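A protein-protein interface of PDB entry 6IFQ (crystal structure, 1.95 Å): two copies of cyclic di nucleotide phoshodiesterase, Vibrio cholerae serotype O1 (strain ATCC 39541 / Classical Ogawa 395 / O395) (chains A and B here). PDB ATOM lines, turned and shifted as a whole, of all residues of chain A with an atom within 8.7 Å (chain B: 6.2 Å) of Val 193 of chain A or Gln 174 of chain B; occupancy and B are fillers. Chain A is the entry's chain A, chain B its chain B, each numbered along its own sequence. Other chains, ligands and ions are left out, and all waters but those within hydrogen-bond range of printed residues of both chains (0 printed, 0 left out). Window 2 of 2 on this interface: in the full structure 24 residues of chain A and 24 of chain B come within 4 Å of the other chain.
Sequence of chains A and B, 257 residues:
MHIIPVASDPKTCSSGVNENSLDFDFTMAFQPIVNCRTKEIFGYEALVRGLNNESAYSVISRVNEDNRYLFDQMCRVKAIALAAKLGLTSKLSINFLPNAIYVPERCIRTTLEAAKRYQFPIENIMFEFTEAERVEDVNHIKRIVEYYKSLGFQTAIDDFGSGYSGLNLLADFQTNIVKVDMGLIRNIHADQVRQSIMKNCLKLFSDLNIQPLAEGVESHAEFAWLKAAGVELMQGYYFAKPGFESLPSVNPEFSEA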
ATOM      1  N   LEU A 184       1.030  38.508  -7.675  1.00  0.00           N
ATOM      2  CA  LEU A 184      -0.132  37.683  -7.354  1.00  0.00           C
ATOM      3  C   LEU A 184      -1.120  37.567  -8.511  1.00  0.00           C
ATOM      4  O   LEU A 184      -2.007  36.705  -8.507  1.00  0.00           O
ATOM      5  CB  LEU A 184      -0.853  38.262  -6.142  1.00  0.00           C
ATOM      6  CG  LEU A 184      -0.054  38.248  -4.849  1.00  0.00           C
ATOM      7  CD1 LEU A 184      -0.945  38.674  -3.714  1.00  0.00           C
ATOM      8  CD2 LEU A 184       0.528  36.845  -4.616  1.00  0.00           C
ATOM      9  N   ASN A 187      -0.636  35.691 -14.671  1.00  0.00           N
ATOM     10  CA  ASN A 187      -1.120  34.403 -15.163  1.00  0.00           C
ATOM     11  C   ASN A 187      -2.076  33.717 -14.184  1.00  0.00           C
ATOM     12  O   ASN A 187      -2.035  32.486 -14.038  1.00  0.00           O
ATOM     13  CB  ASN A 187       0.064  33.459 -15.453  1.00  0.00           C
ATOM     14  CG  ASN A 187       0.893  33.891 -16.656  1.00  0.00           C
ATOM     15  OD1 ASN A 187       0.361  34.391 -17.651  1.00  0.00           O
ATOM     16  ND2 ASN A 187       2.206  33.682 -16.576  1.00  0.00           N
ATOM     17  N   ILE A 188      -2.920  34.497 -13.509  1.00  0.00           N
ATOM     18  CA  ILE A 188      -3.743  33.949 -12.431  1.00  0.00           C
ATOM     19  C   ILE A 188      -4.833  33.019 -12.968  1.00  0.00           C
ATOM     20  O   ILE A 188      -5.285  32.102 -12.286  1.00  0.00           O
ATOM     21  CB  ILE A 188      -4.371  35.065 -11.577  1.00  0.00           C
ATOM     22  CG1 ILE A 188      -5.170  34.480 -10.415  1.00  0.00           C
ATOM     23  CG2 ILE A 188      -5.233  36.003 -12.437  1.00  0.00           C
ATOM     24  CD1 ILE A 188      -5.189  35.403  -9.182  1.00  0.00           C
ATOM     25  N   HIS A 189      -5.234  33.235 -14.209  1.00  0.00           N
ATOM     26  CA  HIS A 189      -6.166  32.329 -14.851  1.00  0.00           C
ATOM     27  C   HIS A 189      -5.573  30.894 -14.933  1.00  0.00           C
ATOM     28  O   HIS A 189      -6.312  29.918 -15.046  1.00  0.00           O
ATOM     29  CB  HIS A 189      -6.517  32.857 -16.251  1.00  0.00           C
ATOM     30  CG  HIS A 189      -5.364  32.823 -17.198  1.00  0.00           C
ATOM     31  ND1 HIS A 189      -4.263  33.640 -17.062  1.00  0.00           N
ATOM     32  CD2 HIS A 189      -5.132  32.058 -18.292  1.00  0.00           C
ATOM     33  CE1 HIS A 189      -3.402  33.380 -18.031  1.00  0.00           C
ATOM     34  NE2 HIS A 189      -3.906  32.425 -18.789  1.00  0.00           N
ATOM     35  N   ALA A 190      -4.247  30.780 -14.816  1.00  0.00           N
ATOM     36  CA  ALA A 190      -3.529  29.519 -15.031  1.00  0.00           C
ATOM     37  C   ALA A 190      -2.999  28.882 -13.758  1.00  0.00           C
ATOM     38  O   ALA A 190      -2.571  27.733 -13.784  1.00  0.00           O
ATOM     39  CB  ALA A 190      -2.365  29.741 -15.987  1.00  0.00           C
ATOM     40  N   ASP A 191      -3.027  29.643 -12.667  1.00  0.00           N
ATOM     41  CA  ASP A 191      -2.288  29.322 -11.460  1.00  0.00           C
ATOM     42  C   ASP A 191      -3.229  29.083 -10.278  1.00  0.00           C
ATOM     43  O   ASP A 191      -3.724  30.014  -9.668  1.00  0.00           O
ATOM     44  CB  ASP A 191      -1.294  30.455 -11.170  1.00  0.00           C
ATOM     45  CG  ASP A 191      -0.327  30.123 -10.050  1.00  0.00           C
ATOM     46  OD1 ASP A 191      -0.750  29.523  -9.051  1.00  0.00           O
ATOM     47  OD2 ASP A 191       0.866  30.472 -10.164  1.00  0.00           O
ATOM     48  N   GLN A 192      -3.436  27.817  -9.939  1.00  0.00           N
ATOM     49  CA  GLN A 192      -4.476  27.443  -8.989  1.00  0.00           C
ATOM     50  C   GLN A 192      -4.158  27.907  -7.563  1.00  0.00           C
ATOM     51  O   GLN A 192      -5.068  28.187  -6.775  1.00  0.00           O
ATOM     52  CB  GLN A 192      -4.698  25.927  -9.015  1.00  0.00           C
ATOM     53  CG  GLN A 192      -3.714  25.146  -9.886  1.00  0.00           C
ATOM     54  CD  GLN A 192      -3.862  25.443 -11.372  1.00  0.00           C
ATOM     55  OE1 GLN A 192      -2.873  25.515 -12.099  1.00  0.00           O
ATOM     56  NE2 GLN A 192      -5.099  25.637 -11.822  1.00  0.00           N
ATOM     57  N   VAL A 193      -2.869  27.981  -7.236  1.00  0.00           N
ATOM     58  CA  VAL A 193      -2.454  28.529  -5.950  1.00  0.00           C
ATOM     59  C   VAL A 193      -2.756  30.035  -5.929  1.00  0.00           C
ATOM     60  O   VAL A 193      -3.363  30.543  -4.982  1.00  0.00           O
ATOM     61  CB  VAL A 193      -0.953  28.251  -5.659  1.00  0.00           C
ATOM     62  CG1 VAL A 193      -0.467  29.044  -4.457  1.00  0.00           C
ATOM     63  CG2 VAL A 193      -0.691  26.707  -5.445  1.00  0.00           C
ATOM     64  N   ARG A 194      -2.374  30.750  -6.989  1.00  0.00           N
ATOM     65  CA  ARG A 194      -2.617  32.191  -7.023  1.00  0.00           C
ATOM     66  C   ARG A 194      -4.122  32.468  -6.949  1.00  0.00           C
ATOM     67  O   ARG A 194      -4.564  33.458  -6.327  1.00  0.00           O
ATOM     68  CB  ARG A 194      -1.990  32.827  -8.272  1.00  0.00           C
ATOM     69  CG  ARG A 194      -0.506  33.146  -8.096  1.00  0.00           C
ATOM     70  CD  ARG A 194       0.117  33.868  -9.312  1.00  0.00           C
ATOM     71  NE  ARG A 194       1.418  34.458  -8.976  1.00  0.00           N
ATOM     72  CZ  ARG A 194       2.512  33.753  -8.678  1.00  0.00           C
ATOM     73  NH1 ARG A 194       2.487  32.430  -8.707  1.00  0.00           N
ATOM     74  NH2 ARG A 194       3.646  34.369  -8.375  1.00  0.00           N
ATOM     75  N   GLN A 195      -4.894  31.547  -7.524  1.00  0.00           N
ATOM     76  CA  GLN A 195      -6.348  31.615  -7.489  1.00  0.00           C
ATOM     77  C   GLN A 195      -6.897  31.517  -6.067  1.00  0.00           C
ATOM     78  O   GLN A 195      -7.782  32.296  -5.713  1.00  0.00           O
ATOM     79  CB  GLN A 195      -6.957  30.515  -8.351  1.00  0.00           C
ATOM     80  CG  GLN A 195      -6.784  30.745  -9.864  1.00  0.00           C
ATOM     81  CD  GLN A 195      -7.354  29.621 -10.707  1.00  0.00           C
ATOM     82  OE1 GLN A 195      -8.179  28.836 -10.245  1.00  0.00           O
ATOM     83  NE2 GLN A 195      -6.911  29.538 -11.958  1.00  0.00           N
ATOM     84  N   SER A 196      -6.402  30.558  -5.264  1.00  0.00           N
ATOM     85  CA  SER A 196      -6.873  30.432  -3.886  1.00  0.00           C
ATOM     86  C   SER A 196      -6.498  31.648  -3.066  1.00  0.00           C
ATOM     87  O   SER A 196      -7.271  32.086  -2.219  1.00  0.00           O
ATOM     88  CB  SER A 196      -6.324  29.167  -3.195  1.00  0.00           C
ATOM     89  OG  SER A 196      -6.868  27.982  -3.763  1.00  0.00           O
ATOM     90  N   ILE A 197      -5.283  32.144  -3.278  1.00  0.00           N
ATOM     91  CA  ILE A 197      -4.798  33.347  -2.597  1.00  0.00           C
ATOM     92  C   ILE A 197      -5.726  34.531  -2.837  1.00  0.00           C
ATOM     93  O   ILE A 197      -6.125  35.213  -1.903  1.00  0.00           O
ATOM     94  CB  ILE A 197      -3.357  33.691  -3.049  1.00  0.00           C
ATOM     95  CG1 ILE A 197      -2.401  32.578  -2.551  1.00  0.00           C
ATOM     96  CG2 ILE A 197      -2.920  35.056  -2.560  1.00  0.00           C
ATOM     97  CD1 ILE A 197      -0.940  32.845  -2.814  1.00  0.00           C
ATOM     98  N   MET A 198      -6.093  34.740  -4.097  1.00  0.00           N
ATOM     99  CA  MET A 198      -6.942  35.846  -4.471  1.00  0.00           C
ATOM    100  C   MET A 198      -8.373  35.602  -3.994  1.00  0.00           C
ATOM    101  O   MET A 198      -8.994  36.504  -3.432  1.00  0.00           O
ATOM    102  CB  MET A 198      -6.882  36.070  -5.982  1.00  0.00           C
ATOM    103  CG  MET A 198      -7.423  37.396  -6.431  1.00  0.00           C
ATOM    104  SD  MET A 198      -6.787  38.798  -5.480  1.00  0.00           S
ATOM    105  CE  MET A 198      -5.020  38.579  -5.607  1.00  0.00           C
ATOM    106  N   LYS A 199      -8.880  34.379  -4.157  1.00  0.00           N
ATOM    107  CA  LYS A 199     -10.222  34.063  -3.661  1.00  0.00           C
ATOM    108  C   LYS A 199     -10.345  34.330  -2.155  1.00  0.00           C
ATOM    109  O   LYS A 199     -11.352  34.858  -1.677  1.00  0.00           O
ATOM    110  CB  LYS A 199     -10.586  32.610  -3.965  1.00  0.00           C
ATOM    111  CG  LYS A 199     -10.926  32.362  -5.444  1.00  0.00           C
ATOM    112  CD  LYS A 199     -11.561  31.001  -5.629  1.00  0.00           C
ATOM    113  CE  LYS A 199     -11.934  30.726  -7.068  1.00  0.00           C
ATOM    114  NZ  LYS A 199     -12.399  29.311  -7.203  1.00  0.00           N
ATOM    115  N   ASN A 200      -9.319  33.971  -1.397  1.00  0.00           N
ATOM    116  CA  ASN A 200      -9.393  34.203   0.034  1.00  0.00           C
ATOM    117  C   ASN A 200      -9.067  35.653   0.428  1.00  0.00           C
ATOM    118  O   ASN A 200      -9.623  36.168   1.392  1.00  0.00           O
ATOM    119  CB  ASN A 200      -8.491  33.195   0.748  1.00  0.00           C
ATOM    120  CG  ASN A 200      -9.078  31.804   0.717  1.00  0.00           C
ATOM    121  OD1 ASN A 200     -10.090  31.539   1.362  1.00  0.00           O
ATOM    122  ND2 ASN A 200      -8.492  30.926  -0.089  1.00  0.00           N
ATOM    123  N   TRP A 225     -10.630  36.404 -15.541  1.00  0.00           N
ATOM    124  CA  TRP A 225     -10.676  35.673 -14.283  1.00  0.00           C
ATOM    125  C   TRP A 225     -10.895  36.639 -13.117  1.00  0.00           C
ATOM    126  O   TRP A 225     -11.821  36.468 -12.311  1.00  0.00           O
ATOM    127  CB  TRP A 225      -9.397  34.871 -14.066  1.00  0.00           C
ATOM    128  CG  TRP A 225      -9.508  33.952 -12.871  1.00  0.00           C
ATOM    129  CD1 TRP A 225      -9.858  32.624 -12.886  1.00  0.00           C
ATOM    130  CD2 TRP A 225      -9.307  34.300 -11.495  1.00  0.00           C
ATOM    131  NE1 TRP A 225      -9.877  32.131 -11.601  1.00  0.00           N
ATOM    132  CE2 TRP A 225      -9.536  33.134 -10.729  1.00  0.00           C
ATOM    133  CE3 TRP A 225      -8.944  35.481 -10.834  1.00  0.00           C
ATOM    134  CZ2 TRP A 225      -9.420  33.115  -9.342  1.00  0.00           C
ATOM    135  CZ3 TRP A 225      -8.830  35.467  -9.459  1.00  0.00           C
ATOM    136  CH2 TRP A 225      -9.060  34.285  -8.723  1.00  0.00           C
ATOM    137  N   LYS B 142      12.842  29.501  -2.536  1.00  0.00           N
ATOM    138  CA  LYS B 142      12.051  28.378  -3.029  1.00  0.00           C
ATOM    139  C   LYS B 142      12.941  27.162  -3.255  1.00  0.00           C
ATOM    140  O   LYS B 142      12.600  26.057  -2.843  1.00  0.00           O
ATOM    141  CB  LYS B 142      11.329  28.746  -4.326  1.00  0.00           C
ATOM    142  CG  LYS B 142      10.580  27.605  -5.003  1.00  0.00           C
ATOM    143  CD  LYS B 142       9.807  28.114  -6.221  1.00  0.00           C
ATOM    144  CE  LYS B 142       9.152  26.988  -7.010  1.00  0.00           C
ATOM    145  NZ  LYS B 142       8.156  26.208  -6.218  1.00  0.00           N
ATOM    146  N   VAL B 145      13.992  25.633   0.080  1.00  0.00           N
ATOM    147  CA  VAL B 145      12.882  24.921   0.705  1.00  0.00           C
ATOM    148  C   VAL B 145      12.570  23.589   0.022  1.00  0.00           C
ATOM    149  O   VAL B 145      12.447  22.554   0.692  1.00  0.00           O
ATOM    150  CB  VAL B 145      11.612  25.776   0.722  1.00  0.00           C
ATOM    151  CG1 VAL B 145      10.425  24.951   1.201  1.00  0.00           C
ATOM    152  CG2 VAL B 145      11.823  26.976   1.616  1.00  0.00           C
ATOM    153  N   GLU B 146      12.437  23.618  -1.302  1.00  0.00           N
ATOM    154  CA  GLU B 146      12.123  22.415  -2.064  1.00  0.00           C
ATOM    155  C   GLU B 146      13.219  21.365  -1.900  1.00  0.00           C
ATOM    156  O   GLU B 146      12.943  20.166  -1.887  1.00  0.00           O
ATOM    157  CB  GLU B 146      11.931  22.747  -3.549  1.00  0.00           C
ATOM    158  CG  GLU B 146      10.738  23.654  -3.856  1.00  0.00           C
ATOM    159  CD  GLU B 146       9.402  22.925  -3.841  1.00  0.00           C
ATOM    160  OE1 GLU B 146       9.372  21.719  -3.509  1.00  0.00           O
ATOM    161  OE2 GLU B 146       8.377  23.563  -4.167  1.00  0.00           O
ATOM    162  N   LYS B 149      12.886  19.737   1.642  1.00  0.00           N
ATOM    163  CA  LYS B 149      11.751  18.828   1.556  1.00  0.00           C
ATOM    164  C   LYS B 149      12.155  17.501   0.913  1.00  0.00           C
ATOM    165  O   LYS B 149      11.694  16.438   1.321  1.00  0.00           O
ATOM    166  CB  LYS B 149      10.617  19.463   0.759  1.00  0.00           C
ATOM    167  CG  LYS B 149       9.285  18.744   0.885  1.00  0.00           C
ATOM    168  CD  LYS B 149       8.963  17.913  -0.348  1.00  0.00           C
ATOM    169  CE  LYS B 149       7.479  17.568  -0.405  1.00  0.00           C
ATOM    170  NZ  LYS B 149       6.635  18.799  -0.556  1.00  0.00           N
ATOM    171  N   THR B 155       9.363  21.851   6.842  1.00  0.00           N
ATOM    172  CA  THR B 155       9.674  23.238   6.532  1.00  0.00           C
ATOM    173  C   THR B 155       8.581  24.157   7.061  1.00  0.00           C
ATOM    174  O   THR B 155       7.417  23.773   7.122  1.00  0.00           O
ATOM    175  CB  THR B 155       9.828  23.475   5.008  1.00  0.00           C
ATOM    176  OG1 THR B 155       8.583  23.208   4.351  1.00  0.00           O
ATOM    177  CG2 THR B 155      10.914  22.581   4.435  1.00  0.00           C
ATOM    178  N   ILE B 157       7.267  28.488   7.054  1.00  0.00           N
ATOM    179  CA  ILE B 157       7.435  29.920   6.959  1.00  0.00           C
ATOM    180  C   ILE B 157       7.165  30.535   8.325  1.00  0.00           C
ATOM    181  O   ILE B 157       6.143  30.270   8.954  1.00  0.00           O
ATOM    182  CB  ILE B 157       6.515  30.542   5.905  1.00  0.00           C
ATOM    183  CG1 ILE B 157       7.011  30.163   4.517  1.00  0.00           C
ATOM    184  CG2 ILE B 157       6.517  32.057   6.045  1.00  0.00           C
ATOM    185  CD1 ILE B 157       5.910  29.853   3.561  1.00  0.00           C
ATOM    186  N   LEU B 169       5.425  34.634  -0.868  1.00  0.00           N
ATOM    187  CA  LEU B 169       6.075  33.370  -0.605  1.00  0.00           C
ATOM    188  C   LEU B 169       5.119  32.240  -0.960  1.00  0.00           C
ATOM    189  O   LEU B 169       5.424  31.407  -1.830  1.00  0.00           O
ATOM    190  CB  LEU B 169       6.518  33.278   0.858  1.00  0.00           C
ATOM    191  CG  LEU B 169       7.569  34.320   1.252  1.00  0.00           C
ATOM    192  CD1 LEU B 169       8.124  34.058   2.647  1.00  0.00           C
ATOM    193  CD2 LEU B 169       8.686  34.373   0.219  1.00  0.00           C
ATOM    194  N   LEU B 170       3.947  32.248  -0.325  1.00  0.00           N
ATOM    195  CA  LEU B 170       2.960  31.191  -0.522  1.00  0.00           C
ATOM    196  C   LEU B 170       2.653  30.976  -1.995  1.00  0.00           C
ATOM    197  O   LEU B 170       2.351  29.863  -2.410  1.00  0.00           O
ATOM    198  CB  LEU B 170       1.657  31.500   0.220  1.00  0.00           C
ATOM    199  CG  LEU B 170       1.690  31.530   1.753  1.00  0.00           C
ATOM    200  CD1 LEU B 170       0.412  30.969   2.339  1.00  0.00           C
ATOM    201  CD2 LEU B 170       2.853  30.758   2.282  1.00  0.00           C
ATOM    202  N   ALA B 171       2.744  32.048  -2.780  1.00  0.00           N
ATOM    203  CA  ALA B 171       2.366  32.007  -4.179  1.00  0.00           C
ATOM    204  C   ALA B 171       3.181  31.033  -5.044  1.00  0.00           C
ATOM    205  O   ALA B 171       2.636  30.449  -5.977  1.00  0.00           O
ATOM    206  CB  ALA B 171       2.454  33.411  -4.776  1.00  0.00           C
ATOM    207  N   ASP B 172       4.470  30.875  -4.761  1.00  0.00           N
ATOM    208  CA  ASP B 172       5.335  30.075  -5.630  1.00  0.00           C
ATOM    209  C   ASP B 172       5.780  28.755  -5.019  1.00  0.00           C
ATOM    210  O   ASP B 172       6.265  27.872  -5.728  1.00  0.00           O
ATOM    211  CB  ASP B 172       6.552  30.896  -6.035  1.00  0.00           C
ATOM    212  CG  ASP B 172       6.206  31.979  -7.054  1.00  0.00           C
ATOM    213  OD1 ASP B 172       5.451  31.675  -8.006  1.00  0.00           O
ATOM    214  OD2 ASP B 172       6.676  33.127  -6.902  1.00  0.00           O
ATOM    215  N   PHE B 173       5.628  28.626  -3.705  1.00  0.00           N
ATOM    216  CA  PHE B 173       5.877  27.348  -3.037  1.00  0.00           C
ATOM    217  C   PHE B 173       5.146  27.302  -1.700  1.00  0.00           C
ATOM    218  O   PHE B 173       4.689  28.334  -1.182  1.00  0.00           O
ATOM    219  CB  PHE B 173       7.379  27.110  -2.833  1.00  0.00           C
ATOM    220  CG  PHE B 173       8.010  28.071  -1.869  1.00  0.00           C
ATOM    221  CD1 PHE B 173       8.466  29.311  -2.301  1.00  0.00           C
ATOM    222  CD2 PHE B 173       8.126  27.749  -0.527  1.00  0.00           C
ATOM    223  CE1 PHE B 173       9.040  30.198  -1.410  1.00  0.00           C
ATOM    224  CE2 PHE B 173       8.694  28.636   0.371  1.00  0.00           C
ATOM    225  CZ  PHE B 173       9.154  29.857  -0.065  1.00  0.00           C
ATOM    226  N   GLN B 174       5.036  26.097  -1.150  1.00  0.00           N
ATOM    227  CA  GLN B 174       4.312  25.873   0.087  1.00  0.00           C
ATOM    228  C   GLN B 174       5.140  25.015   1.044  1.00  0.00           C
ATOM    229  O   GLN B 174       5.637  23.950   0.675  1.00  0.00           O
ATOM    230  CB  GLN B 174       2.954  25.214  -0.197  1.00  0.00           C
ATOM    231  CG  GLN B 174       1.961  26.120  -0.976  1.00  0.00           C
ATOM    232  CD  GLN B 174       2.226  26.126  -2.479  1.00  0.00           C
ATOM    233  OE1 GLN B 174       2.340  27.181  -3.108  1.00  0.00           O
ATOM    234  NE2 GLN B 174       2.322  24.940  -3.057  1.00  0.00           N
ATOM    235  N   THR B 175       5.306  25.508   2.264  1.00  0.00           N
ATOM    236  CA  THR B 175       5.948  24.749   3.337  1.00  0.00           C
ATOM    237  C   THR B 175       4.920  23.822   4.004  1.00  0.00           C
ATOM    238  O   THR B 175       3.720  23.943   3.748  1.00  0.00           O
ATOM    239  CB  THR B 175       6.573  25.716   4.366  1.00  0.00           C
ATOM    240  OG1 THR B 175       5.643  26.780   4.643  1.00  0.00           O
ATOM    241  CG2 THR B 175       7.847  26.343   3.792  1.00  0.00           C
ATOM    242  N   ASN B 176       5.361  22.874   4.836  1.00  0.00           N
ATOM    243  CA  ASN B 176       4.401  22.065   5.594  1.00  0.00           C
ATOM    244  C   ASN B 176       3.589  22.928   6.561  1.00  0.00           C
ATOM    245  O   ASN B 176       2.401  22.700   6.784  1.00  0.00           O
ATOM    246  CB  ASN B 176       5.099  20.969   6.407  1.00  0.00           C
ATOM    247  CG  ASN B 176       6.022  20.114   5.565  1.00  0.00           C
ATOM    248  OD1 ASN B 176       7.225  20.346   5.527  1.00  0.00           O
ATOM    249  ND2 ASN B 176       5.455  19.137   4.869  1.00  0.00           N
ATOM    250  N   LEU B 204      -7.243  29.859   3.421  1.00  0.00           N
ATOM    251  CA  LEU B 204      -6.202  29.837   2.405  1.00  0.00           C
ATOM    252  C   LEU B 204      -5.204  28.689   2.694  1.00  0.00           C
ATOM    253  O   LEU B 204      -4.827  27.947   1.792  1.00  0.00           O
ATOM    254  CB  LEU B 204      -5.482  31.182   2.353  1.00  0.00           C
ATOM    255  CG  LEU B 204      -4.438  31.462   1.272  1.00  0.00           C
ATOM    256  CD1 LEU B 204      -3.049  31.248   1.781  1.00  0.00           C
ATOM    257  CD2 LEU B 204      -4.672  30.621   0.016  1.00  0.00           C
ATOM    258  N   LEU B 208      -4.269  25.341   0.511  1.00  0.00           N
ATOM    259  CA  LEU B 208      -2.899  25.130   0.068  1.00  0.00           C
ATOM    260  C   LEU B 208      -2.228  23.898   0.715  1.00  0.00           C
ATOM    261  O   LEU B 208      -1.028  23.697   0.531  1.00  0.00           O
ATOM    262  CB  LEU B 208      -2.054  26.363   0.361  1.00  0.00           C
ATOM    263  CG  LEU B 208      -2.343  27.543  -0.589  1.00  0.00           C
ATOM    264  CD1 LEU B 208      -1.419  28.707  -0.328  1.00  0.00           C
ATOM    265  CD2 LEU B 208      -2.188  27.058  -1.996  1.00  0.00           C
ATOM    266  N   ASN B 209      -3.004  23.119   1.471  1.00  0.00           N
ATOM    267  CA  ASN B 209      -2.502  21.990   2.273  1.00  0.00           C
ATOM    268  C   ASN B 209      -1.356  22.386   3.221  1.00  0.00           C
ATOM    269  O   ASN B 209      -0.344  21.690   3.333  1.00  0.00           O
ATOM    270  CB  ASN B 209      -2.074  20.833   1.358  1.00  0.00           C
ATOM    271  CG  ASN B 209      -1.908  19.509   2.121  1.00  0.00           C
ATOM    272  OD1 ASN B 209      -2.346  19.376   3.271  1.00  0.00           O
ATOM    273  ND2 ASN B 209      -1.274  18.530   1.479  1.00  0.00           N
ATOM    274  N   ILE B 210      -1.532  23.507   3.916  1.00  0.00           N
ATOM    275  CA  ILE B 210      -0.528  24.021   4.827  1.00  0.00           C
ATOM    276  C   ILE B 210      -1.126  23.997   6.221  1.00  0.00           C
ATOM    277  O   ILE B 210      -2.295  24.341   6.413  1.00  0.00           O
ATOM    278  CB  ILE B 210      -0.068  25.476   4.498  1.00  0.00           C
ATOM    279  CG1 ILE B 210       0.628  25.576   3.144  1.00  0.00           C
ATOM    280  CG2 ILE B 210       0.892  25.971   5.571  1.00  0.00           C
ATOM    281  CD1 ILE B 210       0.931  27.075   2.761  1.00  0.00           C
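Among the printed residues, pairs that only touch across the chains: Asn 200 of chain A with Leu 204 of chain B (3.6 Å), Val 193 of chain A with Leu 170 of chain B (3.6 Å), Val 193 of chain A with Leu 208 of chain B (3.6 Å), Val 193 of chain A with Gln 174 of chain B (3.6 Å), Ile 197 of chain A with Ala 171 of chain B (3.7 Å), Ile 197 of chain A with Leu 204 of chain B (3.7 Å), Ser 196 of chain A with Leu 204 of chain B (3.7 Å), Val 193 of chain A with Ala 171 of chain B (3.7 Å) and Leu 184 of chain A with Ala 171 of chain B (3.9 Å).
No position is printed for both chains. Of the 11 pairs that touch across the chains among the printed residues, none has its exchanged pair printed and touching as well.
Of the 16 printed residues of chain A, 6 touch a printed residue of chain B. Hydrophobic or aromatic side chains of chain A within 4 Å of the printed part of chain B: Leu 184, Val 193 and Ile 197. Among the printed residues, Asp or Glu carboxylates within 4 Å of a Lys or Arg side-chain nitrogen of the other chain: Arg 194 of chain A with Asp 172 of chain B.
Val 193 of chain A touches just these residues of chain B: Leu 170 (3.6 Å), Ala 171 (3.7 Å), Gln 174 (3.6 Å) and Leu 208 (3.6 Å). Printed residues of chain B within 4 Å of Arg 194 of chain A: Ala 171 and Asp 172. Of the printed residues of chain B, Ser 196 of chain A touches Leu 204. Printed residues of chain B within 4 Å of Ile 197 of chain A: Ala 171 (3.7 Å) and Leu 204 (3.7 Å). Thr 155 of chain B touches none of the printed residues of chain A. Of the printed residues of chain A, Leu 170 of chain B touches Val 193 (3.6 Å). Of chain A, only Val 193 (3.6 Å) comes within 4 Å of Gln 174 of chain B. No residue of chain A comes within 4 Å of Thr 175 of chain B. Of the printed residues of chain A, Leu 204 of chain B touches Ser 196, Ile 197 and Asn 200. Asn 209 of chain B touches none of the printed residues of chain A. The nearest residue of chain B that does not touch Val 193 of chain A is Leu 204 of chain B (5.2 Å).
OD1 of Asp 172 of chain B lies within salt-bridge range of NH1 of Arg 194 of chain A. NH1 of Arg 194 of chain A lies within hydrogen-bond range of O of Ala 171 of chain B (3.4 Å).
The backbone carbonyl oxygen (O) of Asp 172 of chain B sits at hydrogen-bond distance from the side-chain amino group (NZ) of Lys 142 of chain B (2.6 Å). NH1 of Arg 194 of chain A lies within salt-bridge range of OD2 of Asp 191 of chain A, 2.9 Å away. The side-chain carboxylate (OD1) of Asp 191 of chain A sits at hydrogen-bond distance from the backbone NH (N) of Val 193 of chain A, at 3.2 Å. The backbone carbonyl oxygen of Leu 170 of chain B lies close to the side-chain amide oxygen of Gln 174 of chain B. O of Ser 196 of chain A is in hydrogen-bond range of ND2 of Asn 200 of chain A (2.7 Å).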
